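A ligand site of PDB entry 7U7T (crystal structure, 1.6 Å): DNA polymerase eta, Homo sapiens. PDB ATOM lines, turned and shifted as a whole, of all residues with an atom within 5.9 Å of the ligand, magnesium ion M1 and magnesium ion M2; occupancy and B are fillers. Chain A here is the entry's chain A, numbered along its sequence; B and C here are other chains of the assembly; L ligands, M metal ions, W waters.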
ATOM      1  N   ASP A  16      -9.488  28.067  -2.906  1.00  0.00           N
ATOM      2  CA  ASP A  16     -10.319  27.617  -4.036  1.00  0.00           C
ATOM      3  C   ASP A  16     -10.890  28.843  -4.761  1.00  0.00           C
ATOM      4  O   ASP A  16     -11.599  29.627  -4.142  1.00  0.00           O
ATOM      5  CB  ASP A  16     -11.386  26.661  -3.552  1.00  0.00           C
ATOM      6  CG  ASP A  16     -12.288  26.183  -4.663  1.00  0.00           C
ATOM      7  OD1 ASP A  16     -11.875  25.326  -5.440  1.00  0.00           O
ATOM      8  OD2 ASP A  16     -13.383  26.704  -4.733  1.00  0.00           O
ATOM      9  N   MET A  17     -10.627  28.912  -6.056  1.00  0.00           N
ATOM     10  CA  MET A  17     -11.151  30.049  -6.839  1.00  0.00           C
ATOM     11  C   MET A  17     -12.678  29.964  -6.902  1.00  0.00           C
ATOM     12  O   MET A  17     -13.207  28.923  -7.187  1.00  0.00           O
ATOM     13  CB  MET A  17     -10.584  30.051  -8.261  1.00  0.00           C
ATOM     14  CG  MET A  17      -9.071  30.005  -8.323  1.00  0.00           C
ATOM     15  SD  MET A  17      -8.246  31.178  -7.242  1.00  0.00           S
ATOM     16  CE  MET A  17      -8.779  32.727  -7.948  1.00  0.00           C
ATOM     17  N   ASP A  18     -13.350  31.084  -6.683  1.00  0.00           N
ATOM     18  CA  ASP A  18     -14.825  31.102  -6.809  1.00  0.00           C
ATOM     19  C   ASP A  18     -15.244  30.937  -8.268  1.00  0.00           C
ATOM     20  O   ASP A  18     -14.623  31.582  -9.098  1.00  0.00           O
ATOM     21  CB  ASP A  18     -15.394  32.394  -6.221  1.00  0.00           C
ATOM     22  CG  ASP A  18     -15.012  32.610  -4.772  1.00  0.00           C
ATOM     23  OD1 ASP A  18     -14.964  31.629  -4.026  1.00  0.00           O
ATOM     24  OD2 ASP A  18     -14.789  33.768  -4.410  1.00  0.00           O
ATOM     25  N   CYS A  19     -16.278  30.124  -8.545  1.00  0.00           N
ATOM     26  CA  CYS A  19     -16.814  29.906  -9.926  1.00  0.00           C
ATOM     27  C   CYS A  19     -15.719  30.184 -10.957  1.00  0.00           C
ATOM     28  O   CYS A  19     -15.914  31.059 -11.766  1.00  0.00           O
ATOM     29  CB  CYS A  19     -18.078  30.738 -10.117  1.00  0.00           C
ATOM     30  SG  CYS A  19     -17.973  32.495  -9.718  1.00  0.00           S
ATOM     31  N   PHE A  20     -14.641  29.399 -10.937  1.00  0.00           N
ATOM     32  CA  PHE A  20     -13.425  29.732 -11.717  1.00  0.00           C
ATOM     33  C   PHE A  20     -13.661  29.994 -13.209  1.00  0.00           C
ATOM     34  O   PHE A  20     -13.327  31.076 -13.653  1.00  0.00           O
ATOM     35  CB  PHE A  20     -12.361  28.652 -11.506  1.00  0.00           C
ATOM     36  CG  PHE A  20     -11.010  29.005 -12.074  1.00  0.00           C
ATOM     37  CD1 PHE A  20     -10.438  30.239 -11.819  1.00  0.00           C
ATOM     38  CD2 PHE A  20     -10.330  28.119 -12.885  1.00  0.00           C
ATOM     39  CE1 PHE A  20      -9.204  30.572 -12.335  1.00  0.00           C
ATOM     40  CE2 PHE A  20      -9.097  28.457 -13.408  1.00  0.00           C
ATOM     41  CZ  PHE A  20      -8.534  29.674 -13.129  1.00  0.00           C
ATOM     42  N   PHE A  21     -14.171  29.006 -13.933  1.00  0.00           N
ATOM     43  CA  PHE A  21     -14.309  29.201 -15.392  1.00  0.00           C
ATOM     44  C   PHE A  21     -15.174  30.431 -15.660  1.00  0.00           C
ATOM     45  O   PHE A  21     -14.893  31.147 -16.611  1.00  0.00           O
ATOM     46  CB  PHE A  21     -14.866  27.944 -16.069  1.00  0.00           C
ATOM     47  CG  PHE A  21     -13.944  26.746 -16.157  1.00  0.00           C
ATOM     48  CD1 PHE A  21     -12.858  26.597 -15.309  1.00  0.00           C
ATOM     49  CD2 PHE A  21     -14.174  25.767 -17.102  1.00  0.00           C
ATOM     50  CE1 PHE A  21     -12.040  25.486 -15.389  1.00  0.00           C
ATOM     51  CE2 PHE A  21     -13.335  24.654 -17.184  1.00  0.00           C
ATOM     52  CZ  PHE A  21     -12.269  24.520 -16.335  1.00  0.00           C
ATOM     53  N   VAL A  22     -16.212  30.641 -14.849  1.00  0.00           N
ATOM     54  CA  VAL A  22     -17.015  31.850 -14.985  1.00  0.00           C
ATOM     55  C   VAL A  22     -16.168  33.092 -14.799  1.00  0.00           C
ATOM     56  O   VAL A  22     -16.244  34.039 -15.595  1.00  0.00           O
ATOM     57  CB  VAL A  22     -18.185  31.815 -13.991  1.00  0.00           C
ATOM     58  CG1 VAL A  22     -18.867  33.205 -13.891  1.00  0.00           C
ATOM     59  CG2 VAL A  22     -19.196  30.762 -14.441  1.00  0.00           C
ATOM     60  N   GLN A  41     -20.263  23.440 -21.974  1.00  0.00           N
ATOM     61  CA  GLN A  41     -19.532  22.805 -23.060  1.00  0.00           C
ATOM     62  C   GLN A  41     -20.502  22.185 -24.037  1.00  0.00           C
ATOM     63  O   GLN A  41     -21.497  21.573 -23.620  1.00  0.00           O
ATOM     64  CB  GLN A  41     -18.409  21.845 -22.570  1.00  0.00           C
ATOM     65  CG  GLN A  41     -18.564  21.271 -21.200  1.00  0.00           C
ATOM     66  CD  GLN A  41     -17.388  20.370 -20.731  1.00  0.00           C
ATOM     67  OE1 GLN A  41     -16.192  20.697 -20.833  1.00  0.00           O
ATOM     68  NE2 GLN A  41     -17.756  19.245 -20.191  1.00  0.00           N
ATOM     69  N   ILE A  51     -20.941  23.622 -16.558  1.00  0.00           N
ATOM     70  CA  ILE A  51     -19.883  23.181 -15.654  1.00  0.00           C
ATOM     71  C   ILE A  51     -19.467  24.225 -14.617  1.00  0.00           C
ATOM     72  O   ILE A  51     -18.751  23.877 -13.679  1.00  0.00           O
ATOM     73  CB  ILE A  51     -18.643  22.683 -16.429  1.00  0.00           C
ATOM     74  CG1 ILE A  51     -18.117  23.773 -17.356  1.00  0.00           C
ATOM     75  CG2 ILE A  51     -18.970  21.359 -17.167  1.00  0.00           C
ATOM     76  CD1 ILE A  51     -16.777  23.388 -17.935  1.00  0.00           C
ATOM     77  N   ALA A  52     -19.921  25.471 -14.726  1.00  0.00           N
ATOM     78  CA  ALA A  52     -19.583  26.498 -13.750  1.00  0.00           C
ATOM     79  C   ALA A  52     -20.685  27.548 -13.730  1.00  0.00           C
ATOM     80  O   ALA A  52     -21.243  27.858 -14.768  1.00  0.00           O
ATOM     81  CB  ALA A  52     -18.229  27.173 -14.059  1.00  0.00           C
ATOM     82  N   VAL A  53     -20.970  28.096 -12.541  1.00  0.00           N
ATOM     83  CA  VAL A  53     -22.137  28.955 -12.323  1.00  0.00           C
ATOM     84  C   VAL A  53     -21.774  30.123 -11.404  1.00  0.00           C
ATOM     85  O   VAL A  53     -21.280  29.914 -10.286  1.00  0.00           O
ATOM     86  CB  VAL A  53     -23.295  28.163 -11.685  1.00  0.00           C
ATOM     87  CG1 VAL A  53     -24.542  29.032 -11.646  1.00  0.00           C
ATOM     88  CG2 VAL A  53     -23.570  26.883 -12.442  1.00  0.00           C
ATOM     89  N   TYR A  55     -22.416  33.145  -8.729  1.00  0.00           N
ATOM     90  CA  TYR A  55     -23.270  33.117  -7.528  1.00  0.00           C
ATOM     91  C   TYR A  55     -24.623  33.790  -7.775  1.00  0.00           C
ATOM     92  O   TYR A  55     -25.648  33.357  -7.205  1.00  0.00           O
ATOM     93  CB  TYR A  55     -22.492  33.713  -6.346  1.00  0.00           C
ATOM     94  CG  TYR A  55     -21.512  32.677  -5.809  1.00  0.00           C
ATOM     95  CD1 TYR A  55     -20.304  32.472  -6.446  1.00  0.00           C
ATOM     96  CD2 TYR A  55     -21.798  31.914  -4.679  1.00  0.00           C
ATOM     97  CE1 TYR A  55     -19.408  31.507  -6.001  1.00  0.00           C
ATOM     98  CE2 TYR A  55     -20.909  30.960  -4.213  1.00  0.00           C
ATOM     99  CZ  TYR A  55     -19.717  30.751  -4.891  1.00  0.00           C
ATOM    100  OH  TYR A  55     -18.801  29.810  -4.466  1.00  0.00           O
ATOM    101  N   ARG A  58     -26.580  31.052  -9.289  1.00  0.00           N
ATOM    102  CA  ARG A  58     -26.902  30.030  -8.294  1.00  0.00           C
ATOM    103  C   ARG A  58     -28.138  30.417  -7.491  1.00  0.00           C
ATOM    104  O   ARG A  58     -28.889  29.542  -7.046  1.00  0.00           O
ATOM    105  CB  ARG A  58     -25.742  29.784  -7.334  1.00  0.00           C
ATOM    106  CG  ARG A  58     -24.467  29.379  -8.039  1.00  0.00           C
ATOM    107  CD  ARG A  58     -23.351  29.162  -7.042  1.00  0.00           C
ATOM    108  NE  ARG A  58     -22.110  28.812  -7.729  1.00  0.00           N
ATOM    109  CZ  ARG A  58     -21.030  28.319  -7.144  1.00  0.00           C
ATOM    110  NH1 ARG A  58     -21.019  28.031  -5.852  1.00  0.00           N
ATOM    111  NH2 ARG A  58     -19.930  28.132  -7.864  1.00  0.00           N
ATOM    112  N   ARG A  64     -24.141  23.247 -11.588  1.00  0.00           N
ATOM    113  CA  ARG A  64     -23.320  22.365 -12.402  1.00  0.00           C
ATOM    114  C   ARG A  64     -24.115  21.111 -12.750  1.00  0.00           C
ATOM    115  O   ARG A  64     -24.969  20.672 -11.991  1.00  0.00           O
ATOM    116  CB  ARG A  64     -22.044  22.043 -11.618  1.00  0.00           C
ATOM    117  CG  ARG A  64     -21.181  20.971 -12.174  1.00  0.00           C
ATOM    118  CD  ARG A  64     -20.184  20.462 -11.118  1.00  0.00           C
ATOM    119  NE  ARG A  64     -19.468  19.335 -11.687  1.00  0.00           N
ATOM    120  CZ  ARG A  64     -19.817  18.064 -11.525  1.00  0.00           C
ATOM    121  NH1 ARG A  64     -20.813  17.703 -10.738  1.00  0.00           N
ATOM    122  NH2 ARG A  64     -19.148  17.125 -12.198  1.00  0.00           N
ATOM    123  N   LEU A  92      -9.744  22.998 -22.997  1.00  0.00           N
ATOM    124  CA  LEU A  92      -9.752  23.784 -21.763  1.00  0.00           C
ATOM    125  C   LEU A  92      -8.473  24.599 -21.557  1.00  0.00           C
ATOM    126  O   LEU A  92      -8.208  25.017 -20.415  1.00  0.00           O
ATOM    127  CB  LEU A  92     -10.004  22.857 -20.559  1.00  0.00           C
ATOM    128  CG  LEU A  92     -11.252  21.970 -20.708  1.00  0.00           C
ATOM    129  CD1 LEU A  92     -11.337  20.951 -19.569  1.00  0.00           C
ATOM    130  CD2 LEU A  92     -12.467  22.852 -20.761  1.00  0.00           C
ATOM    131  N   SER A 116      -6.387  20.699  -7.786  1.00  0.00           N
ATOM    132  CA  SER A 116      -7.209  20.723  -9.007  1.00  0.00           C
ATOM    133  C   SER A 116      -6.857  21.984  -9.807  1.00  0.00           C
ATOM    134  O   SER A 116      -6.014  22.737  -9.378  1.00  0.00           O
ATOM    135  CB  SER A 116      -8.675  20.745  -8.675  1.00  0.00           C
ATOM    136  OG  SER A 116      -9.115  22.030  -8.289  1.00  0.00           O
ATOM    137  N   ILE A 117      -7.543  22.190 -10.931  1.00  0.00           N
ATOM    138  CA  ILE A 117      -7.312  23.396 -11.782  1.00  0.00           C
ATOM    139  C   ILE A 117      -7.484  24.692 -10.968  1.00  0.00           C
ATOM    140  O   ILE A 117      -6.885  25.670 -11.315  1.00  0.00           O
ATOM    141  CB  ILE A 117      -8.243  23.352 -13.025  1.00  0.00           C
ATOM    142  CG1 ILE A 117      -7.733  24.250 -14.148  1.00  0.00           C
ATOM    143  CG2 ILE A 117      -9.684  23.655 -12.668  1.00  0.00           C
ATOM    144  CD1 ILE A 117      -8.317  23.904 -15.499  1.00  0.00           C
ATOM    145  N   ASP A 118      -8.316  24.667  -9.943  1.00  0.00           N
ATOM    146  CA  ASP A 118      -8.623  25.955  -9.256  1.00  0.00           C
ATOM    147  C   ASP A 118      -8.382  25.860  -7.750  1.00  0.00           C
ATOM    148  O   ASP A 118      -8.755  26.804  -7.047  1.00  0.00           O
ATOM    149  CB  ASP A 118     -10.047  26.363  -9.589  1.00  0.00           C
ATOM    150  CG  ASP A 118     -11.078  25.759  -8.660  1.00  0.00           C
ATOM    151  OD1 ASP A 118     -11.021  24.537  -8.415  1.00  0.00           O
ATOM    152  OD2 ASP A 118     -11.924  26.525  -8.187  1.00  0.00           O
ATOM    153  N   GLU A 119      -7.764  24.789  -7.274  1.00  0.00           N
ATOM    154  CA  GLU A 119      -7.503  24.757  -5.821  1.00  0.00           C
ATOM    155  C   GLU A 119      -6.116  24.246  -5.478  1.00  0.00           C
ATOM    156  O   GLU A 119      -5.585  23.397  -6.190  1.00  0.00           O
ATOM    157  CB  GLU A 119      -8.583  23.999  -5.046  1.00  0.00           C
ATOM    158  CG  GLU A 119      -8.599  22.520  -5.197  1.00  0.00           C
ATOM    159  CD  GLU A 119      -9.907  22.039  -4.603  1.00  0.00           C
ATOM    160  OE1 GLU A 119     -10.957  22.307  -5.198  1.00  0.00           O
ATOM    161  OE2 GLU A 119      -9.877  21.493  -3.509  1.00  0.00           O
ATOM    162  N   LYS A 227      -9.962  22.295   3.897  1.00  0.00           N
ATOM    163  CA  LYS A 227     -10.927  22.125   2.810  1.00  0.00           C
ATOM    164  C   LYS A 227     -12.350  22.352   3.297  1.00  0.00           C
ATOM    165  O   LYS A 227     -13.148  23.053   2.646  1.00  0.00           O
ATOM    166  CB  LYS A 227     -10.772  20.716   2.214  1.00  0.00           C
ATOM    167  CG  LYS A 227     -11.813  20.325   1.151  1.00  0.00           C
ATOM    168  CD  LYS A 227     -11.751  21.259  -0.039  1.00  0.00           C
ATOM    169  CE  LYS A 227     -12.658  20.743  -1.167  1.00  0.00           C
ATOM    170  NZ  LYS A 227     -12.609  21.636  -2.350  1.00  0.00           N
ATOM    171  N   LYS A 234     -18.512  31.142   1.464  1.00  0.00           N
ATOM    172  CA  LYS A 234     -18.192  31.416   0.071  1.00  0.00           C
ATOM    173  C   LYS A 234     -19.270  32.354  -0.450  1.00  0.00           C
ATOM    174  O   LYS A 234     -20.415  32.309   0.019  1.00  0.00           O
ATOM    175  CB  LYS A 234     -18.186  30.125  -0.781  1.00  0.00           C
ATOM    176  CG  LYS A 234     -16.816  29.413  -0.919  1.00  0.00           C
ATOM    177  CD  LYS A 234     -16.762  28.465  -2.166  1.00  0.00           C
ATOM    178  CE  LYS A 234     -15.304  28.127  -2.614  1.00  0.00           C
ATOM    179  NZ  LYS A 234     -14.765  28.811  -3.878  1.00  0.00           N
ATOM    180  N   PRO A 235     -18.954  33.233  -1.390  1.00  0.00           N
ATOM    181  CA  PRO A 235     -17.657  33.413  -2.051  1.00  0.00           C
ATOM    182  C   PRO A 235     -16.853  34.540  -1.422  1.00  0.00           C
ATOM    183  O   PRO A 235     -17.379  35.323  -0.608  1.00  0.00           O
ATOM    184  CB  PRO A 235     -18.066  33.811  -3.469  1.00  0.00           C
ATOM    185  CG  PRO A 235     -19.315  34.643  -3.232  1.00  0.00           C
ATOM    186  CD  PRO A 235     -20.021  33.993  -2.061  1.00  0.00           C
ATOM    187  P    DT B   3     -27.870  11.979 -18.998  1.00  0.00           P
ATOM    188  OP1  DT B   3     -28.241  10.554 -18.828  1.00  0.00           O
ATOM    189  OP2  DT B   3     -28.636  13.024 -18.277  1.00  0.00           O
ATOM    190  O5'  DT B   3     -26.333  12.156 -18.625  1.00  0.00           O
ATOM    191  C5'  DT B   3     -25.843  13.391 -18.088  1.00  0.00           C
ATOM    192  C4'  DT B   3     -25.066  14.137 -19.150  1.00  0.00           C
ATOM    193  O4'  DT B   3     -24.570  15.371 -18.563  1.00  0.00           O
ATOM    194  C3'  DT B   3     -23.839  13.390 -19.662  1.00  0.00           C
ATOM    195  O3'  DT B   3     -23.594  13.714 -21.038  1.00  0.00           O
ATOM    196  C2'  DT B   3     -22.742  13.946 -18.777  1.00  0.00           C
ATOM    197  C1'  DT B   3     -23.162  15.399 -18.716  1.00  0.00           C
ATOM    198  N1   DT B   3     -22.599  16.119 -17.568  1.00  0.00           N
ATOM    199  C2   DT B   3     -22.006  17.352 -17.782  1.00  0.00           C
ATOM    200  O2   DT B   3     -21.955  17.893 -18.870  1.00  0.00           O
ATOM    201  N3   DT B   3     -21.486  17.938 -16.648  1.00  0.00           N
ATOM    202  C4   DT B   3     -21.494  17.420 -15.367  1.00  0.00           C
ATOM    203  O4   DT B   3     -20.993  18.063 -14.453  1.00  0.00           O
ATOM    204  C5   DT B   3     -22.129  16.131 -15.220  1.00  0.00           C
ATOM    205  C7   DT B   3     -22.172  15.482 -13.874  1.00  0.00           C
ATOM    206  C6   DT B   3     -22.634  15.550 -16.313  1.00  0.00           C
ATOM    207  P    DT B   4     -22.335  13.066 -21.803  1.00  0.00           P
ATOM    208  OP1  DT B   4     -22.580  13.150 -23.242  1.00  0.00           O
ATOM    209  OP2  DT B   4     -22.030  11.775 -21.154  1.00  0.00           O
ATOM    210  O5'  DT B   4     -21.160  14.075 -21.481  1.00  0.00           O
ATOM    211  C5'  DT B   4     -21.229  15.475 -21.791  1.00  0.00           C
ATOM    212  C4'  DT B   4     -19.874  16.087 -21.568  1.00  0.00           C
ATOM    213  O4'  DT B   4     -19.691  16.396 -20.165  1.00  0.00           O
ATOM    214  C3'  DT B   4     -18.717  15.171 -21.942  1.00  0.00           C
ATOM    215  O3'  DT B   4     -17.813  16.023 -22.638  1.00  0.00           O
ATOM    216  C2'  DT B   4     -18.203  14.677 -20.602  1.00  0.00           C
ATOM    217  C1'  DT B   4     -18.458  15.859 -19.721  1.00  0.00           C
ATOM    218  N1   DT B   4     -18.609  15.534 -18.312  1.00  0.00           N
ATOM    219  C2   DT B   4     -18.096  16.420 -17.389  1.00  0.00           C
ATOM    220  O2   DT B   4     -17.503  17.430 -17.710  1.00  0.00           O
ATOM    221  N3   DT B   4     -18.301  16.069 -16.085  1.00  0.00           N
ATOM    222  C4   DT B   4     -18.978  14.957 -15.611  1.00  0.00           C
ATOM    223  O4   DT B   4     -19.059  14.763 -14.407  1.00  0.00           O
ATOM    224  C5   DT B   4     -19.460  14.062 -16.631  1.00  0.00           C
ATOM    225  C7   DT B   4     -20.175  12.809 -16.214  1.00  0.00           C
ATOM    226  C6   DT B   4     -19.265  14.396 -17.910  1.00  0.00           C
ATOM    227  P    DA B   5     -16.433  15.442 -23.167  1.00  0.00           P
ATOM    228  OP1  DA B   5     -16.144  16.075 -24.460  1.00  0.00           O
ATOM    229  OP2  DA B   5     -16.462  13.983 -23.075  1.00  0.00           O
ATOM    230  O5'  DA B   5     -15.387  16.018 -22.114  1.00  0.00           O
ATOM    231  C5'  DA B   5     -15.195  17.422 -21.952  1.00  0.00           C
ATOM    232  C4'  DA B   5     -14.054  17.684 -20.991  1.00  0.00           C
ATOM    233  O4'  DA B   5     -14.468  17.316 -19.654  1.00  0.00           O
ATOM    234  C3'  DA B   5     -12.790  16.871 -21.291  1.00  0.00           C
ATOM    235  O3'  DA B   5     -11.640  17.697 -21.071  1.00  0.00           O
ATOM    236  C2'  DA B   5     -12.869  15.733 -20.294  1.00  0.00           C
ATOM    237  C1'  DA B   5     -13.561  16.364 -19.112  1.00  0.00           C
ATOM    238  N9   DA B   5     -14.336  15.399 -18.344  1.00  0.00           N
ATOM    239  C8   DA B   5     -14.945  14.275 -18.853  1.00  0.00           C
ATOM    240  N7   DA B   5     -15.574  13.562 -17.949  1.00  0.00           N
ATOM    241  C5   DA B   5     -15.353  14.261 -16.766  1.00  0.00           C
ATOM    242  C6   DA B   5     -15.748  14.018 -15.447  1.00  0.00           C
ATOM    243  N6   DA B   5     -16.481  12.967 -15.075  1.00  0.00           N
ATOM    244  N1   DA B   5     -15.364  14.903 -14.494  1.00  0.00           N
ATOM    245  C2   DA B   5     -14.631  15.960 -14.873  1.00  0.00           C
ATOM    246  N3   DA B   5     -14.187  16.286 -16.080  1.00  0.00           N
ATOM    247  C4   DA B   5     -14.588  15.393 -17.001  1.00  0.00           C
ATOM    248  P    DT C   8     -15.943  17.900  -4.574  1.00  0.00           P
ATOM    249  OP1  DT C   8     -15.582  18.625  -3.338  1.00  0.00           O
ATOM    250  OP2  DT C   8     -17.241  17.195  -4.669  1.00  0.00           O
ATOM    251  O5'  DT C   8     -15.870  18.955  -5.759  1.00  0.00           O
ATOM    252  C5'  DT C   8     -14.837  18.947  -6.768  1.00  0.00           C
ATOM    253  C4'  DT C   8     -15.431  19.216  -8.126  1.00  0.00           C
ATOM    254  O4'  DT C   8     -15.303  18.053  -8.974  1.00  0.00           O
ATOM    255  C3'  DT C   8     -16.925  19.561  -8.113  1.00  0.00           C
ATOM    256  O3'  DT C   8     -17.254  20.634  -9.004  1.00  0.00           O
ATOM    257  C2'  DT C   8     -17.572  18.329  -8.704  1.00  0.00           C
ATOM    258  C1'  DT C   8     -16.507  17.949  -9.696  1.00  0.00           C
ATOM    259  N1   DT C   8     -16.642  16.586 -10.208  1.00  0.00           N
ATOM    260  C2   DT C   8     -16.004  16.275 -11.382  1.00  0.00           C
ATOM    261  O2   DT C   8     -15.245  17.046 -11.957  1.00  0.00           O
ATOM    262  N3   DT C   8     -16.267  15.012 -11.848  1.00  0.00           N
ATOM    263  C4   DT C   8     -17.092  14.072 -11.287  1.00  0.00           C
ATOM    264  O4   DT C   8     -17.218  12.977 -11.819  1.00  0.00           O
ATOM    265  C5   DT C   8     -17.758  14.484 -10.072  1.00  0.00           C
ATOM    266  C7   DT C   8     -18.672  13.525  -9.382  1.00  0.00           C
ATOM    267  C6   DT C   8     -17.518  15.712  -9.605  1.00  0.00           C
HETATM  268  N1  LIG L   1     -16.081  18.956 -16.221  1.00  0.00           N
HETATM  269  C1  LIG L   1     -15.219  19.958 -16.572  1.00  0.00           C
HETATM  270  N2  LIG L   1     -14.721  19.875 -17.818  1.00  0.00           N
HETATM  271  N3  LIG L   1     -14.863  20.997 -15.815  1.00  0.00           N
HETATM  272  C2  LIG L   1     -15.434  20.992 -14.622  1.00  0.00           C
HETATM  273  C3  LIG L   1     -16.296  20.065 -14.136  1.00  0.00           C
HETATM  274  C4  LIG L   1     -16.634  19.005 -14.986  1.00  0.00           C
HETATM  275  O1  LIG L   1     -17.427  18.112 -14.642  1.00  0.00           O
HETATM  276  N4  LIG L   1     -16.699  20.391 -12.847  1.00  0.00           N
HETATM  277  C5  LIG L   1     -16.055  21.520 -12.587  1.00  0.00           C
HETATM  278  N5  LIG L   1     -15.274  21.931 -13.642  1.00  0.00           N
HETATM  279  P1  LIG L   1     -15.029  23.843  -8.665  1.00  0.00           P
HETATM  280  P2  LIG L   1     -16.249  26.498  -9.098  1.00  0.00           P
HETATM  281  P3  LIG L   1     -16.967  27.237  -6.419  1.00  0.00           P
HETATM  282  C6  LIG L   1     -14.464  23.137 -13.785  1.00  0.00           C
HETATM  283  O2  LIG L   1     -14.148  24.418  -7.643  1.00  0.00           O
HETATM  284  O3  LIG L   1     -14.886  27.006  -9.005  1.00  0.00           O
HETATM  285  O4  LIG L   1     -15.636  26.664  -6.082  1.00  0.00           O
HETATM  286  C7  LIG L   1     -15.284  24.421 -13.849  1.00  0.00           C
HETATM  287  O5  LIG L   1     -15.652  22.481  -8.158  1.00  0.00           O
HETATM  288  O6  LIG L   1     -16.935  26.848 -10.427  1.00  0.00           O
HETATM  289  O7  LIG L   1     -17.045  28.735  -6.224  1.00  0.00           O
HETATM  290  C8  LIG L   1     -15.099  25.041 -12.472  1.00  0.00           C
HETATM  291  O8  LIG L   1     -15.137  26.464 -12.602  1.00  0.00           O
HETATM  292  N6  LIG L   1     -16.282  24.855  -8.996  1.00  0.00           N
HETATM  293  O9  LIG L   1     -17.209  27.017  -7.977  1.00  0.00           O
HETATM  294  O10 LIG L   1     -18.163  26.531  -5.737  1.00  0.00           O
HETATM  295  C9  LIG L   1     -13.697  24.555 -12.098  1.00  0.00           C
HETATM  296  O11 LIG L   1     -13.602  23.233 -12.662  1.00  0.00           O
HETATM  297  C10 LIG L   1     -13.397  24.467 -10.614  1.00  0.00           C
HETATM  298  O12 LIG L   1     -14.280  23.501 -10.006  1.00  0.00           O
HETATM  299 MG    MG M   1     -12.125  23.472  -6.663  1.00  0.00          MG
HETATM  300 MG    MG M   2     -13.631  26.710  -7.103  1.00  0.00          MG
HETATM  301  O   HOH W   1     -12.247  21.792  -7.860  1.00  0.00           O
HETATM  302  O   HOH W   2     -15.712  24.435  -4.586  1.00  0.00           O
HETATM  303  O   HOH W   3     -19.737  24.674  -6.592  1.00  0.00           O
HETATM  304  O   HOH W   4     -18.302  23.712 -10.810  1.00  0.00           O
HETATM  305  O   HOH W   5     -12.441  20.804 -11.814  1.00  0.00           O
HETATM  306  O   HOH W   6     -13.779  22.622  -5.228  1.00  0.00           O
HETATM  307  O   HOH W   7     -12.303  18.958 -16.744  1.00  0.00           O
HETATM  308  O   HOH W   8     -19.609  26.920 -10.386  1.00  0.00           O
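O2 of DT 4 of chain B lies within hydrogen-bond range of a nitrogen (N1) of the ligand (2.6 Å). An oxygen (O5) of the ligand lies close to O3' of DT 8 of chain C (2.6 Å). The side-chain hydroxyl (OH) of Tyr 55 sits at hydrogen-bond distance from an oxygen (O7) of the ligand (2.7 Å). The backbone NH of Cys 19 is in hydrogen-bond range of an oxygen (O7) of the ligand. O10 of the ligand lies within salt-bridge range of NH2 of Arg 58 (3.2 Å). An oxygen (O8) of the ligand is in hydrogen-bond range of the backbone NH (N) of Phe 21, 3.0 Å away. The backbone NH of Phe 20 sits at hydrogen-bond distance from an oxygen (O8) of the ligand, 3.4 Å away. An oxygen (O1) of the ligand sits at hydrogen-bond distance from the guanidinium group (NH2) of Arg 64. O4' of DA 5 of chain B sits at hydrogen-bond distance from N2 of the ligand (3.2 Å). N3 of DA 5 of chain B sits at hydrogen-bond distance from N1 of the ligand (3.3 Å). O7 of the ligand lies within salt-bridge range of NZ of Lys 234 (3.3 Å). OE1 of Gln 41 lies within hydrogen-bond range of N2 of the ligand (3.5 Å).
The side-chain hydroxyl (OG) of Ser 116 sits close to the backbone NH (N) of Asp 118. N of Glu 119 lies close to OG of Ser 116. The side-chain amino group of Lys 227 lies within salt-bridge range of the side-chain carboxylate of Glu 119. The side-chain amino group (NZ) of Lys 234 lies within hydrogen-bond range of the backbone carbonyl oxygen (O) of Asp 16, at 3.3 Å. NH2 of Arg 64 is in hydrogen-bond range of N1 of DT 8 of chain C (3.2 Å). OH of Tyr 55 lies within hydrogen-bond range of NH1 of Arg 58. The guanidinium group of Arg 58 sits at hydrogen-bond distance from the backbone carbonyl oxygen of Val 53 (2.9 Å). The side-chain amino group (NZ) of Lys 234 is in salt-bridge range of the side-chain carboxylate (OD1) of Asp 18 (2.8 Å).
Merely in contact with the ligand: Asp 18 (3.3 Å), Ala 52 (3.5 Å), Ile 51 (3.5 Å), DT 3 of chain B (3.6 Å), Ile 117 (3.9 Å) and Leu 92 (3.96 Å). Hydrophobic or aromatic side chains within 4 Å of the ligand: Phe 20, Phe 21, Ile 51, Ala 52, Tyr 55, Leu 92 and Ile 117. Along chain A the residues within 4 Å of the ligand span positions 16 to 234.
Ser 116 touches magnesium ion M1. Four residues have an atom within 4 Å of magnesium ion M1: Asp 16, Ser 116, Asp 118 and Glu 119. The nearest printed residue that does not touch magnesium ion M1 is Lys 227 (4.7 Å).
Within 4 Å of magnesium ion M2: Asp 16, Met 17 and Asp 118. The nearest printed residue that does not touch magnesium ion M2 is Lys 234 (4.01 Å).
Water W1 is bound to magnesium ion M1 (2.1 Å). Magnesium ion M1 is bound by OE1 of Glu 119 (2.2 Å). OD1 of Asp 16 binds magnesium ion M1, 2.2 Å away. The side-chain carboxylate (OD1) of Asp 118 is bound to magnesium ion M1 (2.3 Å). Magnesium ion M1 is bound by water W6 (2.3 Å). Magnesium ion M1 is bound by O2 of the ligand, 2.4 Å away. Magnesium ion M1 has six donor atoms within binding distance.
Magnesium ion M2 is bound by the side-chain carboxylate of Asp 118, an oxygen (O4) of the ligand, the backbone carbonyl oxygen of Met 17, an oxygen (O3) of the ligand, the side-chain carboxylate of Asp 16 and an oxygen (O2) of the ligand. Magnesium ion M2 has six donor atoms within binding distance. Slightly farther from magnesium ion M2 lies the side-chain carboxylate (OD1) of Asp 16 (2.8 Å).
Water W1 lies within hydrogen-bond range of OG of Ser 116 (3.2 Å) and O12 of the ligand (3.4 Å). Water W6 bridges NZ of Lys 227 (3.3 Å) and O5 of the ligand (3.5 Å). Water W8 lies within hydrogen-bond range of O6 of the ligand (2.7 Å), N of Val 53 (2.8 Å) and NH2 of Arg 58 (2.8 Å). Water W7 lies within hydrogen-bond range of a nitrogen (N2) of the ligand and N3 of DA 5 of chain B. Water W4 lies within hydrogen-bond range of the backbone carbonyl oxygen (O) of Ile 51 (2.9 Å) and a nitrogen (N6) of the ligand (2.9 Å).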
